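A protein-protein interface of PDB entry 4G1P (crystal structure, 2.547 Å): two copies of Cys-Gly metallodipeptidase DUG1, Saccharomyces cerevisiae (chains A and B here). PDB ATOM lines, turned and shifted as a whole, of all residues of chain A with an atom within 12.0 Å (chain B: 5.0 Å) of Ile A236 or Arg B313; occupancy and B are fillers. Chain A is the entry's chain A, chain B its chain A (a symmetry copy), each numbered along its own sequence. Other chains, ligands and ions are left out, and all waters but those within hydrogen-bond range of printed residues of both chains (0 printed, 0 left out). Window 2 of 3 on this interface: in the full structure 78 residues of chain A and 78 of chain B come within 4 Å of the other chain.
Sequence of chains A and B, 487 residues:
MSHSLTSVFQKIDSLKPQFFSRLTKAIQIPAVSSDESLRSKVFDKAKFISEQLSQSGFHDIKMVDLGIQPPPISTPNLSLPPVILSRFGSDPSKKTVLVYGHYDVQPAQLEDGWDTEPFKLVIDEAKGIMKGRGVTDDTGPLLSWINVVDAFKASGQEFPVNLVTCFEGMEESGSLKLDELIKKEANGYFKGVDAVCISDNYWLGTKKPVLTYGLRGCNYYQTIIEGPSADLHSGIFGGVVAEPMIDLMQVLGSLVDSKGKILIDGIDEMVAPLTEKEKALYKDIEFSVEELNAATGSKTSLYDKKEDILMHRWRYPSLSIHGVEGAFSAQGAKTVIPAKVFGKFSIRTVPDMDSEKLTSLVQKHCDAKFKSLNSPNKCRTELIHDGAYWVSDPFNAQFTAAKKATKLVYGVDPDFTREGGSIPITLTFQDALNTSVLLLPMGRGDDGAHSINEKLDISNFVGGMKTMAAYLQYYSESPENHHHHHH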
ATOM      1  N   PRO A 228      37.289 -27.157 -23.950  1.00  0.00           N
ATOM      2  CA  PRO A 228      37.919 -26.001 -23.301  1.00  0.00           C
ATOM      3  C   PRO A 228      38.804 -26.455 -22.152  1.00  0.00           C
ATOM      4  O   PRO A 228      38.739 -27.625 -21.741  1.00  0.00           O
ATOM      5  CB  PRO A 228      36.728 -25.242 -22.724  1.00  0.00           C
ATOM      6  CG  PRO A 228      35.720 -26.310 -22.451  1.00  0.00           C
ATOM      7  CD  PRO A 228      35.860 -27.256 -23.613  1.00  0.00           C
ATOM      8  N   ALA A 230      38.734 -25.266 -19.117  1.00  0.00           N
ATOM      9  CA  ALA A 230      37.962 -25.258 -17.886  1.00  0.00           C
ATOM     10  C   ALA A 230      36.478 -25.076 -18.203  1.00  0.00           C
ATOM     11  O   ALA A 230      36.119 -24.743 -19.336  1.00  0.00           O
ATOM     12  CB  ALA A 230      38.452 -24.179 -16.969  1.00  0.00           C
ATOM     13  N   ASP A 231      35.618 -25.323 -17.219  1.00  0.00           N
ATOM     14  CA  ASP A 231      34.183 -25.217 -17.438  1.00  0.00           C
ATOM     15  C   ASP A 231      33.850 -23.821 -17.954  1.00  0.00           C
ATOM     16  O   ASP A 231      34.561 -22.856 -17.675  1.00  0.00           O
ATOM     17  CB  ASP A 231      33.398 -25.539 -16.163  1.00  0.00           C
ATOM     18  CG  ASP A 231      33.353 -27.045 -15.845  1.00  0.00           C
ATOM     19  OD1 ASP A 231      33.834 -27.860 -16.660  1.00  0.00           O
ATOM     20  OD2 ASP A 231      32.825 -27.416 -14.771  1.00  0.00           O
ATOM     21  N   LEU A 232      32.795 -23.722 -18.747  1.00  0.00           N
ATOM     22  CA  LEU A 232      32.432 -22.452 -19.359  1.00  0.00           C
ATOM     23  C   LEU A 232      31.028 -22.073 -18.937  1.00  0.00           C
ATOM     24  O   LEU A 232      30.148 -22.936 -18.830  1.00  0.00           O
ATOM     25  CB  LEU A 232      32.496 -22.538 -20.885  1.00  0.00           C
ATOM     26  CG  LEU A 232      33.858 -22.783 -21.544  1.00  0.00           C
ATOM     27  CD1 LEU A 232      33.733 -22.805 -23.052  1.00  0.00           C
ATOM     28  CD2 LEU A 232      34.874 -21.759 -21.133  1.00  0.00           C
ATOM     29  N   HIS A 233      30.830 -20.786 -18.677  1.00  0.00           N
ATOM     30  CA  HIS A 233      29.503 -20.254 -18.416  1.00  0.00           C
ATOM     31  C   HIS A 233      28.666 -20.553 -19.655  1.00  0.00           C
ATOM     32  O   HIS A 233      29.035 -20.174 -20.762  1.00  0.00           O
ATOM     33  CB  HIS A 233      29.593 -18.747 -18.168  1.00  0.00           C
ATOM     34  CG  HIS A 233      28.297 -18.119 -17.776  1.00  0.00           C
ATOM     35  ND1 HIS A 233      27.223 -18.033 -18.637  1.00  0.00           N
ATOM     36  CD2 HIS A 233      27.899 -17.538 -16.620  1.00  0.00           C
ATOM     37  CE1 HIS A 233      26.218 -17.433 -18.024  1.00  0.00           C
ATOM     38  NE2 HIS A 233      26.602 -17.124 -16.798  1.00  0.00           N
ATOM     39  N   SER A 234      27.557 -21.259 -19.489  1.00  0.00           N
ATOM     40  CA  SER A 234      26.860 -21.750 -20.670  1.00  0.00           C
ATOM     41  C   SER A 234      26.138 -20.644 -21.429  1.00  0.00           C
ATOM     42  O   SER A 234      25.646 -20.884 -22.531  1.00  0.00           O
ATOM     43  CB  SER A 234      25.905 -22.905 -20.351  1.00  0.00           C
ATOM     44  OG  SER A 234      24.700 -22.431 -19.782  1.00  0.00           O
ATOM     45  N   GLY A 235      26.082 -19.450 -20.836  1.00  0.00           N
ATOM     46  CA  GLY A 235      25.417 -18.301 -21.438  1.00  0.00           C
ATOM     47  C   GLY A 235      26.386 -17.453 -22.236  1.00  0.00           C
ATOM     48  O   GLY A 235      26.105 -17.040 -23.350  1.00  0.00           O
ATOM     49  N   ILE A 236      27.555 -17.216 -21.661  1.00  0.00           N
ATOM     50  CA  ILE A 236      28.577 -16.427 -22.314  1.00  0.00           C
ATOM     51  C   ILE A 236      29.090 -17.114 -23.566  1.00  0.00           C
ATOM     52  O   ILE A 236      29.401 -16.464 -24.559  1.00  0.00           O
ATOM     53  CB  ILE A 236      29.751 -16.173 -21.357  1.00  0.00           C
ATOM     54  CG1 ILE A 236      29.258 -15.418 -20.123  1.00  0.00           C
ATOM     55  CG2 ILE A 236      30.863 -15.428 -22.056  1.00  0.00           C
ATOM     56  CD1 ILE A 236      30.311 -15.179 -19.098  1.00  0.00           C
ATOM     57  N   PHE A 237      29.163 -18.435 -23.518  1.00  0.00           N
ATOM     58  CA  PHE A 237      29.783 -19.200 -24.588  1.00  0.00           C
ATOM     59  C   PHE A 237      28.785 -20.076 -25.352  1.00  0.00           C
ATOM     60  O   PHE A 237      29.145 -20.721 -26.326  1.00  0.00           O
ATOM     61  CB  PHE A 237      30.923 -20.047 -24.025  1.00  0.00           C
ATOM     62  CG  PHE A 237      31.993 -19.244 -23.341  1.00  0.00           C
ATOM     63  CD1 PHE A 237      31.881 -18.907 -22.003  1.00  0.00           C
ATOM     64  CD2 PHE A 237      33.116 -18.822 -24.034  1.00  0.00           C
ATOM     65  CE1 PHE A 237      32.870 -18.164 -21.375  1.00  0.00           C
ATOM     66  CE2 PHE A 237      34.103 -18.077 -23.407  1.00  0.00           C
ATOM     67  CZ  PHE A 237      33.977 -17.750 -22.080  1.00  0.00           C
ATOM     68  N   GLY A 238      27.530 -20.085 -24.925  1.00  0.00           N
ATOM     69  CA  GLY A 238      26.525 -20.910 -25.570  1.00  0.00           C
ATOM     70  C   GLY A 238      26.312 -20.598 -27.040  1.00  0.00           C
ATOM     71  O   GLY A 238      26.094 -19.456 -27.408  1.00  0.00           O
ATOM     72  N   GLY A 239      26.367 -21.623 -27.881  1.00  0.00           N
ATOM     73  CA  GLY A 239      26.137 -21.460 -29.300  1.00  0.00           C
ATOM     74  C   GLY A 239      27.403 -21.096 -30.057  1.00  0.00           C
ATOM     75  O   GLY A 239      27.387 -20.900 -31.274  1.00  0.00           O
ATOM     76  N   VAL A 240      28.517 -21.024 -29.350  1.00  0.00           N
ATOM     77  CA  VAL A 240      29.720 -20.475 -29.960  1.00  0.00           C
ATOM     78  C   VAL A 240      30.958 -21.353 -29.790  1.00  0.00           C
ATOM     79  O   VAL A 240      31.860 -21.312 -30.608  1.00  0.00           O
ATOM     80  CB  VAL A 240      29.953 -19.034 -29.437  1.00  0.00           C
ATOM     81  CG1 VAL A 240      31.259 -18.918 -28.670  1.00  0.00           C
ATOM     82  CG2 VAL A 240      29.862 -18.032 -30.581  1.00  0.00           C
ATOM     83  N   VAL A 241      30.990 -22.151 -28.724  1.00  0.00           N
ATOM     84  CA  VAL A 241      32.033 -23.159 -28.520  1.00  0.00           C
ATOM     85  C   VAL A 241      31.404 -24.538 -28.568  1.00  0.00           C
ATOM     86  O   VAL A 241      30.234 -24.706 -28.238  1.00  0.00           O
ATOM     87  CB  VAL A 241      32.726 -22.995 -27.162  1.00  0.00           C
ATOM     88  CG1 VAL A 241      33.181 -21.544 -26.974  1.00  0.00           C
ATOM     89  CG2 VAL A 241      31.785 -23.377 -26.046  1.00  0.00           C
ATOM     90  N   ALA A 242      32.164 -25.532 -28.996  1.00  0.00           N
ATOM     91  CA  ALA A 242      31.619 -26.876 -29.080  1.00  0.00           C
ATOM     92  C   ALA A 242      31.551 -27.493 -27.676  1.00  0.00           C
ATOM     93  O   ALA A 242      32.435 -27.254 -26.839  1.00  0.00           O
ATOM     94  CB  ALA A 242      32.450 -27.716 -29.995  1.00  0.00           C
ATOM     95  N   GLU A 243      30.504 -28.276 -27.413  1.00  0.00           N
ATOM     96  CA  GLU A 243      30.299 -28.833 -26.078  1.00  0.00           C
ATOM     97  C   GLU A 243      30.578 -30.343 -26.004  1.00  0.00           C
ATOM     98  O   GLU A 243      29.912 -31.144 -26.669  1.00  0.00           O
ATOM     99  CB  GLU A 243      28.887 -28.521 -25.582  1.00  0.00           C
ATOM    100  CG  GLU A 243      28.507 -27.054 -25.724  1.00  0.00           C
ATOM    101  CD  GLU A 243      27.181 -26.691 -25.053  1.00  0.00           C
ATOM    102  OE1 GLU A 243      26.612 -27.520 -24.302  1.00  0.00           O
ATOM    103  OE2 GLU A 243      26.695 -25.567 -25.284  1.00  0.00           O
ATOM    104  N   LYS A 334      22.329 -25.988 -13.092  1.00  0.00           N
ATOM    105  CA  LYS A 334      23.618 -25.326 -13.195  1.00  0.00           C
ATOM    106  C   LYS A 334      23.912 -25.000 -14.670  1.00  0.00           C
ATOM    107  O   LYS A 334      23.914 -25.878 -15.540  1.00  0.00           O
ATOM    108  CB  LYS A 334      24.724 -26.187 -12.586  1.00  0.00           C
ATOM    109  CG  LYS A 334      26.060 -25.463 -12.325  1.00  0.00           C
ATOM    110  CD  LYS A 334      27.113 -26.454 -11.858  1.00  0.00           C
ATOM    111  CE  LYS A 334      28.329 -25.814 -11.175  1.00  0.00           C
ATOM    112  NZ  LYS A 334      28.939 -26.737 -10.130  1.00  0.00           N
ATOM    113  N   THR A 335      24.139 -23.723 -14.943  1.00  0.00           N
ATOM    114  CA  THR A 335      24.333 -23.257 -16.304  1.00  0.00           C
ATOM    115  C   THR A 335      25.800 -23.287 -16.617  1.00  0.00           C
ATOM    116  O   THR A 335      26.488 -22.259 -16.548  1.00  0.00           O
ATOM    117  CB  THR A 335      23.835 -21.833 -16.487  1.00  0.00           C
ATOM    118  OG1 THR A 335      24.178 -21.065 -15.334  1.00  0.00           O
ATOM    119  CG2 THR A 335      22.339 -21.805 -16.662  1.00  0.00           C
ATOM    120  N   VAL A 336      26.273 -24.471 -16.983  1.00  0.00           N
ATOM    121  CA  VAL A 336      27.689 -24.676 -17.233  1.00  0.00           C
ATOM    122  C   VAL A 336      27.921 -25.581 -18.442  1.00  0.00           C
ATOM    123  O   VAL A 336      27.144 -26.489 -18.717  1.00  0.00           O
ATOM    124  CB  VAL A 336      28.385 -25.277 -15.979  1.00  0.00           C
ATOM    125  CG1 VAL A 336      27.752 -26.610 -15.602  1.00  0.00           C
ATOM    126  CG2 VAL A 336      29.859 -25.436 -16.219  1.00  0.00           C
ATOM    127  N   ILE A 337      28.988 -25.306 -19.174  1.00  0.00           N
ATOM    128  CA  ILE A 337      29.455 -26.186 -20.225  1.00  0.00           C
ATOM    129  C   ILE A 337      30.657 -26.939 -19.671  1.00  0.00           C
ATOM    130  O   ILE A 337      31.737 -26.369 -19.526  1.00  0.00           O
ATOM    131  CB  ILE A 337      29.853 -25.370 -21.466  1.00  0.00           C
ATOM    132  CG1 ILE A 337      28.620 -24.702 -22.076  1.00  0.00           C
ATOM    133  CG2 ILE A 337      30.529 -26.233 -22.497  1.00  0.00           C
ATOM    134  CD1 ILE A 337      28.911 -23.885 -23.313  1.00  0.00           C
ATOM    135  N   PRO A 338      30.470 -28.225 -19.327  1.00  0.00           N
ATOM    136  CA  PRO A 338      31.588 -29.008 -18.767  1.00  0.00           C
ATOM    137  C   PRO A 338      32.754 -29.099 -19.734  1.00  0.00           C
ATOM    138  O   PRO A 338      32.532 -29.216 -20.935  1.00  0.00           O
ATOM    139  CB  PRO A 338      30.966 -30.386 -18.523  1.00  0.00           C
ATOM    140  CG  PRO A 338      29.468 -30.085 -18.338  1.00  0.00           C
ATOM    141  CD  PRO A 338      29.188 -28.964 -19.296  1.00  0.00           C
ATOM    142  N   TYR B 202      29.895  -8.695 -18.044  1.00  0.00           N
ATOM    143  CA  TYR B 202      31.329  -8.531 -18.309  1.00  0.00           C
ATOM    144  C   TYR B 202      31.547  -7.874 -19.645  1.00  0.00           C
ATOM    145  O   TYR B 202      30.647  -7.863 -20.481  1.00  0.00           O
ATOM    146  CB  TYR B 202      32.015  -9.905 -18.311  1.00  0.00           C
ATOM    147  CG  TYR B 202      31.325 -10.840 -17.365  1.00  0.00           C
ATOM    148  CD1 TYR B 202      30.250 -11.622 -17.790  1.00  0.00           C
ATOM    149  CD2 TYR B 202      31.681 -10.881 -16.024  1.00  0.00           C
ATOM    150  CE1 TYR B 202      29.574 -12.445 -16.904  1.00  0.00           C
ATOM    151  CE2 TYR B 202      31.018 -11.701 -15.138  1.00  0.00           C
ATOM    152  CZ  TYR B 202      29.966 -12.482 -15.575  1.00  0.00           C
ATOM    153  OH  TYR B 202      29.297 -13.297 -14.683  1.00  0.00           O
ATOM    154  N   LEU B 204      32.962  -7.801 -23.356  1.00  0.00           N
ATOM    155  CA  LEU B 204      32.983  -8.852 -24.359  1.00  0.00           C
ATOM    156  C   LEU B 204      34.310  -9.618 -24.346  1.00  0.00           C
ATOM    157  O   LEU B 204      34.349 -10.848 -24.422  1.00  0.00           O
ATOM    158  CB  LEU B 204      32.767  -8.217 -25.729  1.00  0.00           C
ATOM    159  CG  LEU B 204      32.916  -9.141 -26.923  1.00  0.00           C
ATOM    160  CD1 LEU B 204      31.832 -10.181 -26.844  1.00  0.00           C
ATOM    161  CD2 LEU B 204      32.812  -8.311 -28.195  1.00  0.00           C
ATOM    162  N   ARG B 216      20.177 -12.337 -23.357  1.00  0.00           N
ATOM    163  CA  ARG B 216      19.391 -13.505 -23.707  1.00  0.00           C
ATOM    164  C   ARG B 216      18.667 -13.976 -22.467  1.00  0.00           C
ATOM    165  O   ARG B 216      19.163 -13.812 -21.360  1.00  0.00           O
ATOM    166  CB  ARG B 216      20.287 -14.637 -24.138  1.00  0.00           C
ATOM    167  CG  ARG B 216      20.883 -14.546 -25.488  1.00  0.00           C
ATOM    168  CD  ARG B 216      22.101 -15.397 -25.414  1.00  0.00           C
ATOM    169  NE  ARG B 216      22.289 -16.286 -26.536  1.00  0.00           N
ATOM    170  CZ  ARG B 216      23.282 -17.163 -26.608  1.00  0.00           C
ATOM    171  NH1 ARG B 216      24.143 -17.263 -25.609  1.00  0.00           N
ATOM    172  NH2 ARG B 216      23.414 -17.932 -27.678  1.00  0.00           N
ATOM    173  N   PHE B 287      36.361  -7.575 -31.868  1.00  0.00           N
ATOM    174  CA  PHE B 287      36.425  -8.944 -31.372  1.00  0.00           C
ATOM    175  C   PHE B 287      36.923  -9.898 -32.439  1.00  0.00           C
ATOM    176  O   PHE B 287      36.664  -9.711 -33.626  1.00  0.00           O
ATOM    177  CB  PHE B 287      35.064  -9.417 -30.890  1.00  0.00           C
ATOM    178  CG  PHE B 287      35.122 -10.654 -30.058  1.00  0.00           C
ATOM    179  CD1 PHE B 287      35.719 -10.631 -28.809  1.00  0.00           C
ATOM    180  CD2 PHE B 287      34.569 -11.837 -30.511  1.00  0.00           C
ATOM    181  CE1 PHE B 287      35.769 -11.771 -28.029  1.00  0.00           C
ATOM    182  CE2 PHE B 287      34.613 -12.982 -29.742  1.00  0.00           C
ATOM    183  CZ  PHE B 287      35.211 -12.950 -28.499  1.00  0.00           C
ATOM    184  N   LEU B 292      38.285 -15.302 -28.405  1.00  0.00           N
ATOM    185  CA  LEU B 292      37.427 -16.384 -27.951  1.00  0.00           C
ATOM    186  C   LEU B 292      38.255 -17.613 -27.549  1.00  0.00           C
ATOM    187  O   LEU B 292      38.039 -18.189 -26.493  1.00  0.00           O
ATOM    188  CB  LEU B 292      36.414 -16.754 -29.028  1.00  0.00           C
ATOM    189  CG  LEU B 292      35.464 -17.893 -28.661  1.00  0.00           C
ATOM    190  CD1 LEU B 292      34.577 -17.450 -27.506  1.00  0.00           C
ATOM    191  CD2 LEU B 292      34.634 -18.311 -29.871  1.00  0.00           C
ATOM    192  N   ASP B 308      29.658 -13.695 -36.935  1.00  0.00           N
ATOM    193  CA  ASP B 308      29.009 -14.951 -36.584  1.00  0.00           C
ATOM    194  C   ASP B 308      29.138 -15.276 -35.108  1.00  0.00           C
ATOM    195  O   ASP B 308      28.146 -15.613 -34.455  1.00  0.00           O
ATOM    196  CB  ASP B 308      29.563 -16.090 -37.427  1.00  0.00           C
ATOM    197  CG  ASP B 308      29.003 -16.089 -38.832  1.00  0.00           C
ATOM    198  OD1 ASP B 308      27.796 -15.770 -38.981  1.00  0.00           O
ATOM    199  OD2 ASP B 308      29.775 -16.401 -39.772  1.00  0.00           O
ATOM    200  N   ILE B 309      30.361 -15.179 -34.592  1.00  0.00           N
ATOM    201  CA  ILE B 309      30.594 -15.384 -33.175  1.00  0.00           C
ATOM    202  C   ILE B 309      29.685 -14.457 -32.381  1.00  0.00           C
ATOM    203  O   ILE B 309      29.021 -14.878 -31.436  1.00  0.00           O
ATOM    204  CB  ILE B 309      32.040 -15.092 -32.792  1.00  0.00           C
ATOM    205  CG1 ILE B 309      32.993 -16.012 -33.550  1.00  0.00           C
ATOM    206  CG2 ILE B 309      32.224 -15.275 -31.306  1.00  0.00           C
ATOM    207  CD1 ILE B 309      34.440 -15.557 -33.524  1.00  0.00           C
ATOM    208  N   LEU B 310      29.627 -13.193 -32.789  1.00  0.00           N
ATOM    209  CA  LEU B 310      28.858 -12.230 -32.024  1.00  0.00           C
ATOM    210  C   LEU B 310      27.368 -12.542 -32.098  1.00  0.00           C
ATOM    211  O   LEU B 310      26.677 -12.552 -31.075  1.00  0.00           O
ATOM    212  CB  LEU B 310      29.175 -10.792 -32.447  1.00  0.00           C
ATOM    213  CG  LEU B 310      30.631 -10.334 -32.268  1.00  0.00           C
ATOM    214  CD1 LEU B 310      30.863  -8.984 -32.920  1.00  0.00           C
ATOM    215  CD2 LEU B 310      31.058 -10.295 -30.805  1.00  0.00           C
ATOM    216  N   MET B 311      26.878 -12.835 -33.295  1.00  0.00           N
ATOM    217  CA  MET B 311      25.448 -13.061 -33.463  1.00  0.00           C
ATOM    218  C   MET B 311      24.963 -14.358 -32.832  1.00  0.00           C
ATOM    219  O   MET B 311      23.818 -14.447 -32.371  1.00  0.00           O
ATOM    220  CB  MET B 311      25.045 -12.977 -34.932  1.00  0.00           C
ATOM    221  CG  MET B 311      25.033 -11.546 -35.454  1.00  0.00           C
ATOM    222  SD  MET B 311      24.210 -11.433 -37.039  1.00  0.00           S
ATOM    223  CE  MET B 311      25.090 -12.704 -37.944  1.00  0.00           C
ATOM    224  N   HIS B 312      25.838 -15.352 -32.791  1.00  0.00           N
ATOM    225  CA  HIS B 312      25.489 -16.597 -32.139  1.00  0.00           C
ATOM    226  C   HIS B 312      25.641 -16.554 -30.614  1.00  0.00           C
ATOM    227  O   HIS B 312      25.024 -17.360 -29.919  1.00  0.00           O
ATOM    228  CB  HIS B 312      26.209 -17.785 -32.783  1.00  0.00           C
ATOM    229  CG  HIS B 312      25.561 -18.237 -34.054  1.00  0.00           C
ATOM    230  ND1 HIS B 312      26.076 -17.952 -35.300  1.00  0.00           N
ATOM    231  CD2 HIS B 312      24.403 -18.905 -34.269  1.00  0.00           C
ATOM    232  CE1 HIS B 312      25.276 -18.444 -36.228  1.00  0.00           C
ATOM    233  NE2 HIS B 312      24.253 -19.026 -35.628  1.00  0.00           N
ATOM    234  N   ARG B 313      26.431 -15.610 -30.094  1.00  0.00           N
ATOM    235  CA  ARG B 313      26.396 -15.318 -28.656  1.00  0.00           C
ATOM    236  C   ARG B 313      25.211 -14.447 -28.274  1.00  0.00           C
ATOM    237  O   ARG B 313      24.704 -14.561 -27.169  1.00  0.00           O
ATOM    238  CB  ARG B 313      27.633 -14.565 -28.189  1.00  0.00           C
ATOM    239  CG  ARG B 313      28.933 -15.236 -28.452  1.00  0.00           C
ATOM    240  CD  ARG B 313      30.055 -14.248 -28.209  1.00  0.00           C
ATOM    241  NE  ARG B 313      30.233 -13.997 -26.787  1.00  0.00           N
ATOM    242  CZ  ARG B 313      31.394 -14.114 -26.165  1.00  0.00           C
ATOM    243  NH1 ARG B 313      32.467 -14.458 -26.855  1.00  0.00           N
ATOM    244  NH2 ARG B 313      31.485 -13.876 -24.863  1.00  0.00           N
ATOM    245  N   TRP B 314      24.791 -13.552 -29.166  1.00  0.00           N
ATOM    246  CA  TRP B 314      23.874 -12.479 -28.762  1.00  0.00           C
ATOM    247  C   TRP B 314      22.412 -12.611 -29.175  1.00  0.00           C
ATOM    248  O   TRP B 314      21.523 -12.241 -28.410  1.00  0.00           O
ATOM    249  CB  TRP B 314      24.388 -11.117 -29.232  1.00  0.00           C
ATOM    250  CG  TRP B 314      25.670 -10.689 -28.601  1.00  0.00           C
ATOM    251  CD1 TRP B 314      26.284 -11.255 -27.524  1.00  0.00           C
ATOM    252  CD2 TRP B 314      26.512  -9.604 -29.023  1.00  0.00           C
ATOM    253  NE1 TRP B 314      27.455 -10.597 -27.255  1.00  0.00           N
ATOM    254  CE2 TRP B 314      27.618  -9.576 -28.155  1.00  0.00           C
ATOM    255  CE3 TRP B 314      26.434  -8.654 -30.055  1.00  0.00           C
ATOM    256  CZ2 TRP B 314      28.640  -8.629 -28.277  1.00  0.00           C
ATOM    257  CZ3 TRP B 314      27.451  -7.721 -30.180  1.00  0.00           C
ATOM    258  CH2 TRP B 314      28.539  -7.715 -29.295  1.00  0.00           C
ATOM    259  N   ARG B 315      22.149 -13.098 -30.385  1.00  0.00           N
ATOM    260  CA  ARG B 315      20.798 -12.954 -30.927  1.00  0.00           C
ATOM    261  C   ARG B 315      20.227 -14.193 -31.595  1.00  0.00           C
ATOM    262  O   ARG B 315      19.091 -14.171 -32.042  1.00  0.00           O
ATOM    263  CB  ARG B 315      20.708 -11.741 -31.869  1.00  0.00           C
ATOM    264  CG  ARG B 315      21.621 -11.815 -33.079  1.00  0.00           C
ATOM    265  CD  ARG B 315      20.841 -12.209 -34.319  1.00  0.00           C
ATOM    266  NE  ARG B 315      19.678 -11.354 -34.500  1.00  0.00           N
ATOM    267  CZ  ARG B 315      18.490 -11.787 -34.908  1.00  0.00           C
ATOM    268  NH1 ARG B 315      18.316 -13.070 -35.189  1.00  0.00           N
ATOM    269  NH2 ARG B 315      17.472 -10.939 -35.040  1.00  0.00           N
ATOM    270  N   GLU B 419      24.535  -9.389 -24.562  1.00  0.00           N
ATOM    271  CA  GLU B 419      25.074 -10.410 -23.671  1.00  0.00           C
ATOM    272  C   GLU B 419      24.533 -11.787 -24.015  1.00  0.00           C
ATOM    273  O   GLU B 419      23.327 -11.954 -24.255  1.00  0.00           O
ATOM    274  CB  GLU B 419      24.703 -10.106 -22.222  1.00  0.00           C
ATOM    275  CG  GLU B 419      25.861  -9.725 -21.342  1.00  0.00           C
ATOM    276  CD  GLU B 419      26.895 -10.820 -21.206  1.00  0.00           C
ATOM    277  OE1 GLU B 419      26.505 -11.994 -21.022  1.00  0.00           O
ATOM    278  OE2 GLU B 419      28.104 -10.494 -21.281  1.00  0.00           O
ATOM    279  N   GLY B 420      25.429 -12.769 -24.017  1.00  0.00           N
ATOM    280  CA  GLY B 420      25.033 -14.161 -24.120  1.00  0.00           C
ATOM    281  C   GLY B 420      24.403 -14.636 -22.824  1.00  0.00           C
ATOM    282  O   GLY B 420      23.521 -15.494 -22.816  1.00  0.00           O
ATOM    283  N   GLY B 421      24.858 -14.062 -21.715  1.00  0.00           N
ATOM    284  CA  GLY B 421      24.346 -14.419 -20.407  1.00  0.00           C
ATOM    285  C   GLY B 421      22.979 -13.823 -20.150  1.00  0.00           C
ATOM    286  O   GLY B 421      22.397 -13.197 -21.039  1.00  0.00           O
ATOM    287  N   GLY B 445      35.610 -10.634 -19.942  1.00  0.00           N
ATOM    288  CA  GLY B 445      34.890 -11.805 -20.407  1.00  0.00           C
ATOM    289  C   GLY B 445      35.604 -13.113 -20.135  1.00  0.00           C
ATOM    290  O   GLY B 445      35.107 -14.178 -20.495  1.00  0.00           O
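The backbone carbonyl oxygen of Gly A235 is in hydrogen-bond range of the guanidinium group of Arg B216, at 3.0 Å. O of Ile A236 lies close to NH2 of Arg B313 (3.3 Å). O of Gly A238 is in hydrogen-bond range of NH2 of Arg B216 (3.1 Å). O of Gly A235 lies close to O of Gly B420, at 3.1 Å. O of Gly A238 lies close to O of His B312, 3.4 Å away.
A ring nitrogen (ND1) of His A233 is in hydrogen-bond range of the backbone NH (N) of Gly A235, at 2.9 Å. ND1 of His A233 is in hydrogen-bond range of N of Ile A236 (3.1 Å). NH2 of Arg B216 is in hydrogen-bond range of O of His B312 (2.8 Å). The guanidinium group (NE) of Arg B216 lies close to the backbone carbonyl oxygen (O) of Arg B313 (3.0 Å). N of Arg B216 sits at hydrogen-bond distance from O of Glu B419 (3.3 Å). The side-chain carboxylate of Glu B419 sits at hydrogen-bond distance from the backbone NH of Gly B421 (2.7 Å).
Among the printed residues, merely in contact across the chains: Gly A235 with Gly B421, Ile A236 with Tyr B202, Gly A239 with His B312, Val A240 with Leu B292, Val A240 with Ile B309 and Val A240 with Arg B313.
Ile A236 touches just these residues of chain B: Tyr B202 (3.6 Å) and Arg B313 (3.3 Å). Of chain A, only Ile A236 (3.3 Å) and Val A240 (3.6 Å) come within 4 Å of Arg B313. Ile B309 touches just one residue of chain A: Val A240. No residue of chain A comes within 4 Å of Trp B314. No residue of chain A comes within 4 Å of Glu B419. Of chain A, only Gly A235 (3.0 Å) comes within 4 Å of Gly B420. Of chain A, only Gly A235 (3.6 Å) comes within 4 Å of Gly B421. No residue of chain A comes within 4 Å of Gly B445. Of the printed residues of chain A, Leu B292 touches Val A240. Printed residues of chain B within 4 Å of Gly A235: Arg B216, Gly B420 and Gly B421. Printed residues of chain B within 4 Å of Gly A238: Arg B216 and His B312. Thr A335 touches none of the printed residues of chain B. Ala A242 touches none of the printed residues of chain B. The nearest residue of chain B that does not touch Ile A236 is Gly B421 (4.2 Å). The nearest residue of chain A that does not touch Arg B313 is Gly A238 (4.3 Å). The nearest printed residue of chain B that does not touch Gly A235 is Arg B313 (4.8 Å).
Along chain A the printed residues that touch a printed residue of chain B span positions 235 to 240. Among the printed residues, 11 pairs touch across the chains.
No position is printed for both chains.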
